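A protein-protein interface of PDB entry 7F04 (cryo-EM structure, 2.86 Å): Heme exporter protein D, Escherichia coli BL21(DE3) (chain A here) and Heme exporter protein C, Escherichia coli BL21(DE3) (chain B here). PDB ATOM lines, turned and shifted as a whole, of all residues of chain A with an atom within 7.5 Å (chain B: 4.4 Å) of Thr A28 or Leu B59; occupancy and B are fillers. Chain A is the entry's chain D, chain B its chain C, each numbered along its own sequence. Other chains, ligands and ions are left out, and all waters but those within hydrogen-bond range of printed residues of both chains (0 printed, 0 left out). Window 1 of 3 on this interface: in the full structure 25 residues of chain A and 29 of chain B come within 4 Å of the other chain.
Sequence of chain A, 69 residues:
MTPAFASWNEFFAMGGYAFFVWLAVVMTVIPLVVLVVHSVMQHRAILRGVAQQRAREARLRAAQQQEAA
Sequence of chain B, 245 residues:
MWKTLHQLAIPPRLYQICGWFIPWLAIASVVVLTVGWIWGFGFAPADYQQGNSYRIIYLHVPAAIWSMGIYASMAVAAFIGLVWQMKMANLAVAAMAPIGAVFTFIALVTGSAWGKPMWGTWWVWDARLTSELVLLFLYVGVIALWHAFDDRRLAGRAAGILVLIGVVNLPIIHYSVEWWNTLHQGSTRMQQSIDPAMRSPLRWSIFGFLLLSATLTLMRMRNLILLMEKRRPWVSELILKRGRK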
ATOM      1  N   VAL A  21      -8.730  -2.773 -18.990  1.00  0.00           N
ATOM      2  CA  VAL A  21      -8.539  -3.390 -20.297  1.00  0.00           C
ATOM      3  C   VAL A  21      -8.145  -4.851 -20.142  1.00  0.00           C
ATOM      4  O   VAL A  21      -8.722  -5.739 -20.778  1.00  0.00           O
ATOM      5  CB  VAL A  21      -7.493  -2.609 -21.109  1.00  0.00           C
ATOM      6  CG1 VAL A  21      -6.939  -3.473 -22.226  1.00  0.00           C
ATOM      7  CG2 VAL A  21      -8.104  -1.338 -21.670  1.00  0.00           C
ATOM      8  N   TRP A  22      -7.164  -5.125 -19.285  1.00  0.00           N
ATOM      9  CA  TRP A  22      -6.650  -6.479 -19.141  1.00  0.00           C
ATOM     10  C   TRP A  22      -7.561  -7.374 -18.319  1.00  0.00           C
ATOM     11  O   TRP A  22      -7.505  -8.597 -18.477  1.00  0.00           O
ATOM     12  CB  TRP A  22      -5.251  -6.444 -18.529  1.00  0.00           C
ATOM     13  CG  TRP A  22      -4.236  -5.830 -19.443  1.00  0.00           C
ATOM     14  CD1 TRP A  22      -3.449  -4.751 -19.183  1.00  0.00           C
ATOM     15  CD2 TRP A  22      -3.911  -6.251 -20.773  1.00  0.00           C
ATOM     16  NE1 TRP A  22      -2.650  -4.476 -20.262  1.00  0.00           N
ATOM     17  CE2 TRP A  22      -2.915  -5.384 -21.252  1.00  0.00           C
ATOM     18  CE3 TRP A  22      -4.362  -7.282 -21.602  1.00  0.00           C
ATOM     19  CZ2 TRP A  22      -2.362  -5.513 -22.522  1.00  0.00           C
ATOM     20  CZ3 TRP A  22      -3.813  -7.408 -22.860  1.00  0.00           C
ATOM     21  CH2 TRP A  22      -2.823  -6.530 -23.308  1.00  0.00           C
ATOM     22  N   LEU A  23      -8.384  -6.806 -17.437  1.00  0.00           N
ATOM     23  CA  LEU A  23      -9.388  -7.619 -16.761  1.00  0.00           C
ATOM     24  C   LEU A  23     -10.402  -8.157 -17.757  1.00  0.00           C
ATOM     25  O   LEU A  23     -10.822  -9.315 -17.662  1.00  0.00           O
ATOM     26  CB  LEU A  23     -10.087  -6.811 -15.670  1.00  0.00           C
ATOM     27  CG  LEU A  23     -11.251  -7.509 -14.968  1.00  0.00           C
ATOM     28  CD1 LEU A  23     -10.758  -8.703 -14.170  1.00  0.00           C
ATOM     29  CD2 LEU A  23     -11.998  -6.540 -14.073  1.00  0.00           C
ATOM     30  N   ALA A  24     -10.809  -7.330 -18.722  1.00  0.00           N
ATOM     31  CA  ALA A  24     -11.714  -7.797 -19.764  1.00  0.00           C
ATOM     32  C   ALA A  24     -11.053  -8.857 -20.632  1.00  0.00           C
ATOM     33  O   ALA A  24     -11.681  -9.863 -20.981  1.00  0.00           O
ATOM     34  CB  ALA A  24     -12.185  -6.621 -20.616  1.00  0.00           C
ATOM     35  N   VAL A  25      -9.780  -8.658 -20.980  1.00  0.00           N
ATOM     36  CA  VAL A  25      -9.071  -9.619 -21.821  1.00  0.00           C
ATOM     37  C   VAL A  25      -8.976 -10.969 -21.122  1.00  0.00           C
ATOM     38  O   VAL A  25      -9.283 -12.015 -21.703  1.00  0.00           O
ATOM     39  CB  VAL A  25      -7.676  -9.082 -22.184  1.00  0.00           C
ATOM     40  CG1 VAL A  25      -6.822 -10.187 -22.772  1.00  0.00           C
ATOM     41  CG2 VAL A  25      -7.781  -7.909 -23.137  1.00  0.00           C
ATOM     42  N   VAL A  26      -8.556 -10.961 -19.857  1.00  0.00           N
ATOM     43  CA  VAL A  26      -8.432 -12.204 -19.104  1.00  0.00           C
ATOM     44  C   VAL A  26      -9.796 -12.851 -18.916  1.00  0.00           C
ATOM     45  O   VAL A  26      -9.956 -14.066 -19.088  1.00  0.00           O
ATOM     46  CB  VAL A  26      -7.740 -11.933 -17.755  1.00  0.00           C
ATOM     47  CG1 VAL A  26      -7.992 -13.072 -16.783  1.00  0.00           C
ATOM     48  CG2 VAL A  26      -6.251 -11.717 -17.959  1.00  0.00           C
ATOM     49  N   MET A  27     -10.800 -12.051 -18.568  1.00  0.00           N
ATOM     50  CA  MET A  27     -12.121 -12.557 -18.233  1.00  0.00           C
ATOM     51  C   MET A  27     -12.926 -12.953 -19.466  1.00  0.00           C
ATOM     52  O   MET A  27     -13.999 -13.545 -19.324  1.00  0.00           O
ATOM     53  CB  MET A  27     -12.858 -11.501 -17.398  1.00  0.00           C
ATOM     54  CG  MET A  27     -14.210 -11.913 -16.849  1.00  0.00           C
ATOM     55  SD  MET A  27     -14.081 -13.283 -15.685  1.00  0.00           S
ATOM     56  CE  MET A  27     -13.351 -12.457 -14.275  1.00  0.00           C
ATOM     57  N   THR A  28     -12.445 -12.638 -20.668  1.00  0.00           N
ATOM     58  CA  THR A  28     -13.019 -13.214 -21.877  1.00  0.00           C
ATOM     59  C   THR A  28     -12.219 -14.393 -22.409  1.00  0.00           C
ATOM     60  O   THR A  28     -12.805 -15.305 -22.998  1.00  0.00           O
ATOM     61  CB  THR A  28     -13.139 -12.165 -22.988  1.00  0.00           C
ATOM     62  OG1 THR A  28     -13.862 -12.723 -24.090  1.00  0.00           O
ATOM     63  CG2 THR A  28     -11.778 -11.772 -23.491  1.00  0.00           C
ATOM     64  N   VAL A  29     -10.898 -14.401 -22.216  1.00  0.00           N
ATOM     65  CA  VAL A  29     -10.090 -15.523 -22.675  1.00  0.00           C
ATOM     66  C   VAL A  29     -10.355 -16.752 -21.821  1.00  0.00           C
ATOM     67  O   VAL A  29     -10.442 -17.874 -22.333  1.00  0.00           O
ATOM     68  CB  VAL A  29      -8.600 -15.135 -22.678  1.00  0.00           C
ATOM     69  CG1 VAL A  29      -7.720 -16.369 -22.682  1.00  0.00           C
ATOM     70  CG2 VAL A  29      -8.290 -14.254 -23.873  1.00  0.00           C
ATOM     71  N   ILE A  30     -10.506 -16.563 -20.509  1.00  0.00           N
ATOM     72  CA  ILE A  30     -10.679 -17.703 -19.609  1.00  0.00           C
ATOM     73  C   ILE A  30     -11.935 -18.512 -19.922  1.00  0.00           C
ATOM     74  O   ILE A  30     -11.834 -19.744 -20.023  1.00  0.00           O
ATOM     75  CB  ILE A  30     -10.617 -17.234 -18.146  1.00  0.00           C
ATOM     76  CG1 ILE A  30      -9.169 -16.950 -17.747  1.00  0.00           C
ATOM     77  CG2 ILE A  30     -11.233 -18.271 -17.224  1.00  0.00           C
ATOM     78  CD1 ILE A  30      -8.993 -16.600 -16.289  1.00  0.00           C
ATOM     79  N   PRO A  31     -13.125 -17.916 -20.072  1.00  0.00           N
ATOM     80  CA  PRO A  31     -14.301 -18.749 -20.381  1.00  0.00           C
ATOM     81  C   PRO A  31     -14.236 -19.418 -21.744  1.00  0.00           C
ATOM     82  O   PRO A  31     -14.725 -20.544 -21.885  1.00  0.00           O
ATOM     83  CB  PRO A  31     -15.477 -17.766 -20.292  1.00  0.00           C
ATOM     84  CG  PRO A  31     -14.956 -16.569 -19.619  1.00  0.00           C
ATOM     85  CD  PRO A  31     -13.498 -16.505 -19.900  1.00  0.00           C
ATOM     86  N   LEU A  32     -13.652 -18.767 -22.750  1.00  0.00           N
ATOM     87  CA  LEU A  32     -13.515 -19.406 -24.055  1.00  0.00           C
ATOM     88  C   LEU A  32     -12.592 -20.615 -23.983  1.00  0.00           C
ATOM     89  O   LEU A  32     -12.899 -21.679 -24.541  1.00  0.00           O
ATOM     90  CB  LEU A  32     -12.998 -18.397 -25.078  1.00  0.00           C
ATOM     91  CG  LEU A  32     -13.939 -17.247 -25.430  1.00  0.00           C
ATOM     92  CD1 LEU A  32     -13.258 -16.272 -26.371  1.00  0.00           C
ATOM     93  CD2 LEU A  32     -15.226 -17.771 -26.040  1.00  0.00           C
ATOM     94  N   VAL A  33     -11.457 -20.472 -23.297  1.00  0.00           N
ATOM     95  CA  VAL A  33     -10.539 -21.592 -23.133  1.00  0.00           C
ATOM     96  C   VAL A  33     -11.191 -22.689 -22.307  1.00  0.00           C
ATOM     97  O   VAL A  33     -10.985 -23.880 -22.558  1.00  0.00           O
ATOM     98  CB  VAL A  33      -9.216 -21.112 -22.509  1.00  0.00           C
ATOM     99  CG1 VAL A  33      -8.314 -22.290 -22.194  1.00  0.00           C
ATOM    100  CG2 VAL A  33      -8.514 -20.152 -23.448  1.00  0.00           C
ATOM    101  N   VAL A  34     -11.993 -22.308 -21.312  1.00  0.00           N
ATOM    102  CA  VAL A  34     -12.706 -23.299 -20.514  1.00  0.00           C
ATOM    103  C   VAL A  34     -13.678 -24.081 -21.384  1.00  0.00           C
ATOM    104  O   VAL A  34     -13.775 -25.306 -21.279  1.00  0.00           O
ATOM    105  CB  VAL A  34     -13.420 -22.626 -19.329  1.00  0.00           C
ATOM    106  CG1 VAL A  34     -14.495 -23.537 -18.773  1.00  0.00           C
ATOM    107  CG2 VAL A  34     -12.420 -22.278 -18.244  1.00  0.00           C
ATOM    108  N   PHE B  41      -6.355  -3.793 -30.525  1.00  0.00           N
ATOM    109  CA  PHE B  41      -5.560  -4.091 -29.335  1.00  0.00           C
ATOM    110  C   PHE B  41      -4.067  -3.937 -29.615  1.00  0.00           C
ATOM    111  O   PHE B  41      -3.265  -4.827 -29.328  1.00  0.00           O
ATOM    112  CB  PHE B  41      -5.863  -5.499 -28.818  1.00  0.00           C
ATOM    113  CG  PHE B  41      -6.954  -5.554 -27.797  1.00  0.00           C
ATOM    114  CD1 PHE B  41      -6.787  -4.974 -26.555  1.00  0.00           C
ATOM    115  CD2 PHE B  41      -8.143  -6.201 -28.076  1.00  0.00           C
ATOM    116  CE1 PHE B  41      -7.790  -5.030 -25.612  1.00  0.00           C
ATOM    117  CE2 PHE B  41      -9.148  -6.260 -27.139  1.00  0.00           C
ATOM    118  CZ  PHE B  41      -8.973  -5.675 -25.904  1.00  0.00           C
ATOM    119  N   ILE B  56     -11.924  -2.217 -25.937  1.00  0.00           N
ATOM    120  CA  ILE B  56     -12.780  -3.351 -25.610  1.00  0.00           C
ATOM    121  C   ILE B  56     -13.905  -3.530 -26.618  1.00  0.00           C
ATOM    122  O   ILE B  56     -14.680  -4.485 -26.501  1.00  0.00           O
ATOM    123  CB  ILE B  56     -13.309  -3.182 -24.173  1.00  0.00           C
ATOM    124  CG1 ILE B  56     -12.177  -2.724 -23.254  1.00  0.00           C
ATOM    125  CG2 ILE B  56     -13.862  -4.486 -23.628  1.00  0.00           C
ATOM    126  CD1 ILE B  56     -12.624  -2.358 -21.860  1.00  0.00           C
ATOM    127  N   ILE B  57     -14.012  -2.653 -27.621  1.00  0.00           N
ATOM    128  CA  ILE B  57     -14.970  -2.888 -28.698  1.00  0.00           C
ATOM    129  C   ILE B  57     -14.699  -4.233 -29.349  1.00  0.00           C
ATOM    130  O   ILE B  57     -15.597  -5.071 -29.483  1.00  0.00           O
ATOM    131  CB  ILE B  57     -14.926  -1.753 -29.741  1.00  0.00           C
ATOM    132  CG1 ILE B  57     -13.486  -1.367 -30.079  1.00  0.00           C
ATOM    133  CG2 ILE B  57     -15.733  -0.560 -29.297  1.00  0.00           C
ATOM    134  CD1 ILE B  57     -13.380  -0.377 -31.208  1.00  0.00           C
ATOM    135  N   TYR B  58     -13.437  -4.477 -29.713  1.00  0.00           N
ATOM    136  CA  TYR B  58     -13.069  -5.668 -30.464  1.00  0.00           C
ATOM    137  C   TYR B  58     -13.320  -6.930 -29.666  1.00  0.00           C
ATOM    138  O   TYR B  58     -13.324  -8.028 -30.231  1.00  0.00           O
ATOM    139  CB  TYR B  58     -11.595  -5.598 -30.844  1.00  0.00           C
ATOM    140  CG  TYR B  58     -11.166  -4.246 -31.344  1.00  0.00           C
ATOM    141  CD1 TYR B  58     -11.549  -3.791 -32.592  1.00  0.00           C
ATOM    142  CD2 TYR B  58     -10.361  -3.430 -30.569  1.00  0.00           C
ATOM    143  CE1 TYR B  58     -11.154  -2.554 -33.047  1.00  0.00           C
ATOM    144  CE2 TYR B  58      -9.957  -2.197 -31.017  1.00  0.00           C
ATOM    145  CZ  TYR B  58     -10.356  -1.763 -32.256  1.00  0.00           C
ATOM    146  OH  TYR B  58      -9.956  -0.528 -32.708  1.00  0.00           O
ATOM    147  N   LEU B  59     -13.521  -6.789 -28.364  1.00  0.00           N
ATOM    148  CA  LEU B  59     -13.605  -7.905 -27.444  1.00  0.00           C
ATOM    149  C   LEU B  59     -14.955  -8.016 -26.755  1.00  0.00           C
ATOM    150  O   LEU B  59     -15.362  -9.120 -26.395  1.00  0.00           O
ATOM    151  CB  LEU B  59     -12.475  -7.777 -26.417  1.00  0.00           C
ATOM    152  CG  LEU B  59     -12.137  -8.836 -25.390  1.00  0.00           C
ATOM    153  CD1 LEU B  59     -10.680  -8.705 -25.052  1.00  0.00           C
ATOM    154  CD2 LEU B  59     -12.941  -8.558 -24.160  1.00  0.00           C
ATOM    155  N   HIS B  60     -15.663  -6.902 -26.576  1.00  0.00           N
ATOM    156  CA  HIS B  60     -16.997  -6.888 -25.988  1.00  0.00           C
ATOM    157  C   HIS B  60     -18.107  -6.882 -27.028  1.00  0.00           C
ATOM    158  O   HIS B  60     -19.122  -7.558 -26.842  1.00  0.00           O
ATOM    159  CB  HIS B  60     -17.157  -5.670 -25.074  1.00  0.00           C
ATOM    160  CG  HIS B  60     -18.576  -5.233 -24.884  1.00  0.00           C
ATOM    161  ND1 HIS B  60     -19.433  -5.848 -23.998  1.00  0.00           N
ATOM    162  CD2 HIS B  60     -19.285  -4.233 -25.457  1.00  0.00           C
ATOM    163  CE1 HIS B  60     -20.609  -5.250 -24.038  1.00  0.00           C
ATOM    164  NE2 HIS B  60     -20.546  -4.268 -24.916  1.00  0.00           N
ATOM    165  N   VAL B  61     -17.945  -6.120 -28.114  1.00  0.00           N
ATOM    166  CA  VAL B  61     -18.994  -6.054 -29.132  1.00  0.00           C
ATOM    167  C   VAL B  61     -19.231  -7.393 -29.816  1.00  0.00           C
ATOM    168  O   VAL B  61     -20.403  -7.774 -29.982  1.00  0.00           O
ATOM    169  CB  VAL B  61     -18.685  -4.921 -30.131  1.00  0.00           C
ATOM    170  CG1 VAL B  61     -19.738  -4.882 -31.218  1.00  0.00           C
ATOM    171  CG2 VAL B  61     -18.631  -3.592 -29.407  1.00  0.00           C
ATOM    172  N   PRO B  62     -18.208  -8.140 -30.261  1.00  0.00           N
ATOM    173  CA  PRO B  62     -18.498  -9.432 -30.905  1.00  0.00           C
ATOM    174  C   PRO B  62     -19.258 -10.399 -30.019  1.00  0.00           C
ATOM    175  O   PRO B  62     -20.151 -11.101 -30.505  1.00  0.00           O
ATOM    176  CB  PRO B  62     -17.102  -9.963 -31.255  1.00  0.00           C
ATOM    177  CG  PRO B  62     -16.261  -8.763 -31.352  1.00  0.00           C
ATOM    178  CD  PRO B  62     -16.765  -7.846 -30.297  1.00  0.00           C
ATOM    179  N   ALA B  63     -18.937 -10.453 -28.727  1.00  0.00           N
ATOM    180  CA  ALA B  63     -19.659 -11.342 -27.825  1.00  0.00           C
ATOM    181  C   ALA B  63     -21.112 -10.917 -27.680  1.00  0.00           C
ATOM    182  O   ALA B  63     -22.015 -11.760 -27.683  1.00  0.00           O
ATOM    183  CB  ALA B  63     -18.972 -11.377 -26.462  1.00  0.00           C
ATOM    184  N   ILE B 106     -19.673 -13.038 -21.168  1.00  0.00           N
ATOM    185  CA  ILE B 106     -18.523 -12.249 -21.599  1.00  0.00           C
ATOM    186  C   ILE B 106     -18.946 -10.822 -21.912  1.00  0.00           C
ATOM    187  O   ILE B 106     -18.264  -9.864 -21.537  1.00  0.00           O
ATOM    188  CB  ILE B 106     -17.837 -12.918 -22.804  1.00  0.00           C
ATOM    189  CG1 ILE B 106     -17.041 -14.141 -22.350  1.00  0.00           C
ATOM    190  CG2 ILE B 106     -16.925 -11.937 -23.509  1.00  0.00           C
ATOM    191  CD1 ILE B 106     -16.517 -14.982 -23.486  1.00  0.00           C
ATOM    192  N   THR B 110     -17.539  -7.696 -19.784  1.00  0.00           N
ATOM    193  CA  THR B 110     -16.702  -6.768 -20.521  1.00  0.00           C
ATOM    194  C   THR B 110     -17.342  -5.401 -20.672  1.00  0.00           C
ATOM    195  O   THR B 110     -16.626  -4.417 -20.876  1.00  0.00           O
ATOM    196  CB  THR B 110     -16.381  -7.334 -21.902  1.00  0.00           C
ATOM    197  OG1 THR B 110     -17.580  -7.835 -22.499  1.00  0.00           O
ATOM    198  CG2 THR B 110     -15.407  -8.476 -21.765  1.00  0.00           C
ATOM    199  N   PHE B 209     -15.357 -14.314 -33.815  1.00  0.00           N
ATOM    200  CA  PHE B 209     -16.264 -14.918 -32.843  1.00  0.00           C
ATOM    201  C   PHE B 209     -17.310 -15.782 -33.528  1.00  0.00           C
ATOM    202  O   PHE B 209     -17.729 -16.805 -32.979  1.00  0.00           O
ATOM    203  CB  PHE B 209     -16.938 -13.858 -31.973  1.00  0.00           C
ATOM    204  CG  PHE B 209     -16.071 -13.337 -30.866  1.00  0.00           C
ATOM    205  CD1 PHE B 209     -16.522 -13.365 -29.559  1.00  0.00           C
ATOM    206  CD2 PHE B 209     -14.821 -12.811 -31.124  1.00  0.00           C
ATOM    207  CE1 PHE B 209     -15.741 -12.891 -28.532  1.00  0.00           C
ATOM    208  CE2 PHE B 209     -14.036 -12.333 -30.101  1.00  0.00           C
ATOM    209  CZ  PHE B 209     -14.497 -12.372 -28.803  1.00  0.00           C
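A ring nitrogen (ND1) of His B60 is in hydrogen-bond range of the side-chain hydroxyl (OG1) of Thr B110.
Among the printed residues, merely in contact across the chains: Thr A28 with Ile B106, Thr A28 with Leu B59, Val A25 with Leu B59, Ala A24 with Leu B59, Val A25 with Phe B41, Val A21 with Phe B41, Ala A24 with Thr B110 and Leu A32 with Ile B106.
Of the printed residues of chain B, Ala A24 touches Leu B59 and Thr B110. Thr A28 touches just these residues of chain B: Leu B59 (3.5 Å) and Ile B106 (3.2 Å). Printed residues of chain A within 4 Å of Phe B41: Val A21 and Val A25. Of chain A, only Ala A24, Val A25 and Thr A28 come within 4 Å of Leu B59. Of the printed residues of chain A, Ile B106 touches Thr A28 and Leu A32. Phe B209 touches none of the printed residues of chain A. The nearest residue of chain A that does not touch Leu B59 is Val A21 (5.6 Å). The nearest printed residue of chain A that does not touch Thr B110 is Thr A28 (4.5 Å).
Printed residues of chain A that touch a printed residue of chain B: Val A21, Ala A24, Val A25, Thr A28 and Leu A32. Hydrophobic or aromatic side chains of chain A that line the printed part of chain B: Val A21, Ala A24, Val A25 and Leu A32. Printed residues of chain B that touch a printed residue of chain A: Phe B41, Leu B59, Ile B106 and Thr B110. Along chain B the printed residues that touch a printed residue of chain A span positions 41 to 110. Among the printed residues, no Asp or Glu carboxylate lies within 4 Å of a Lys or Arg side-chain nitrogen of the other chain.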
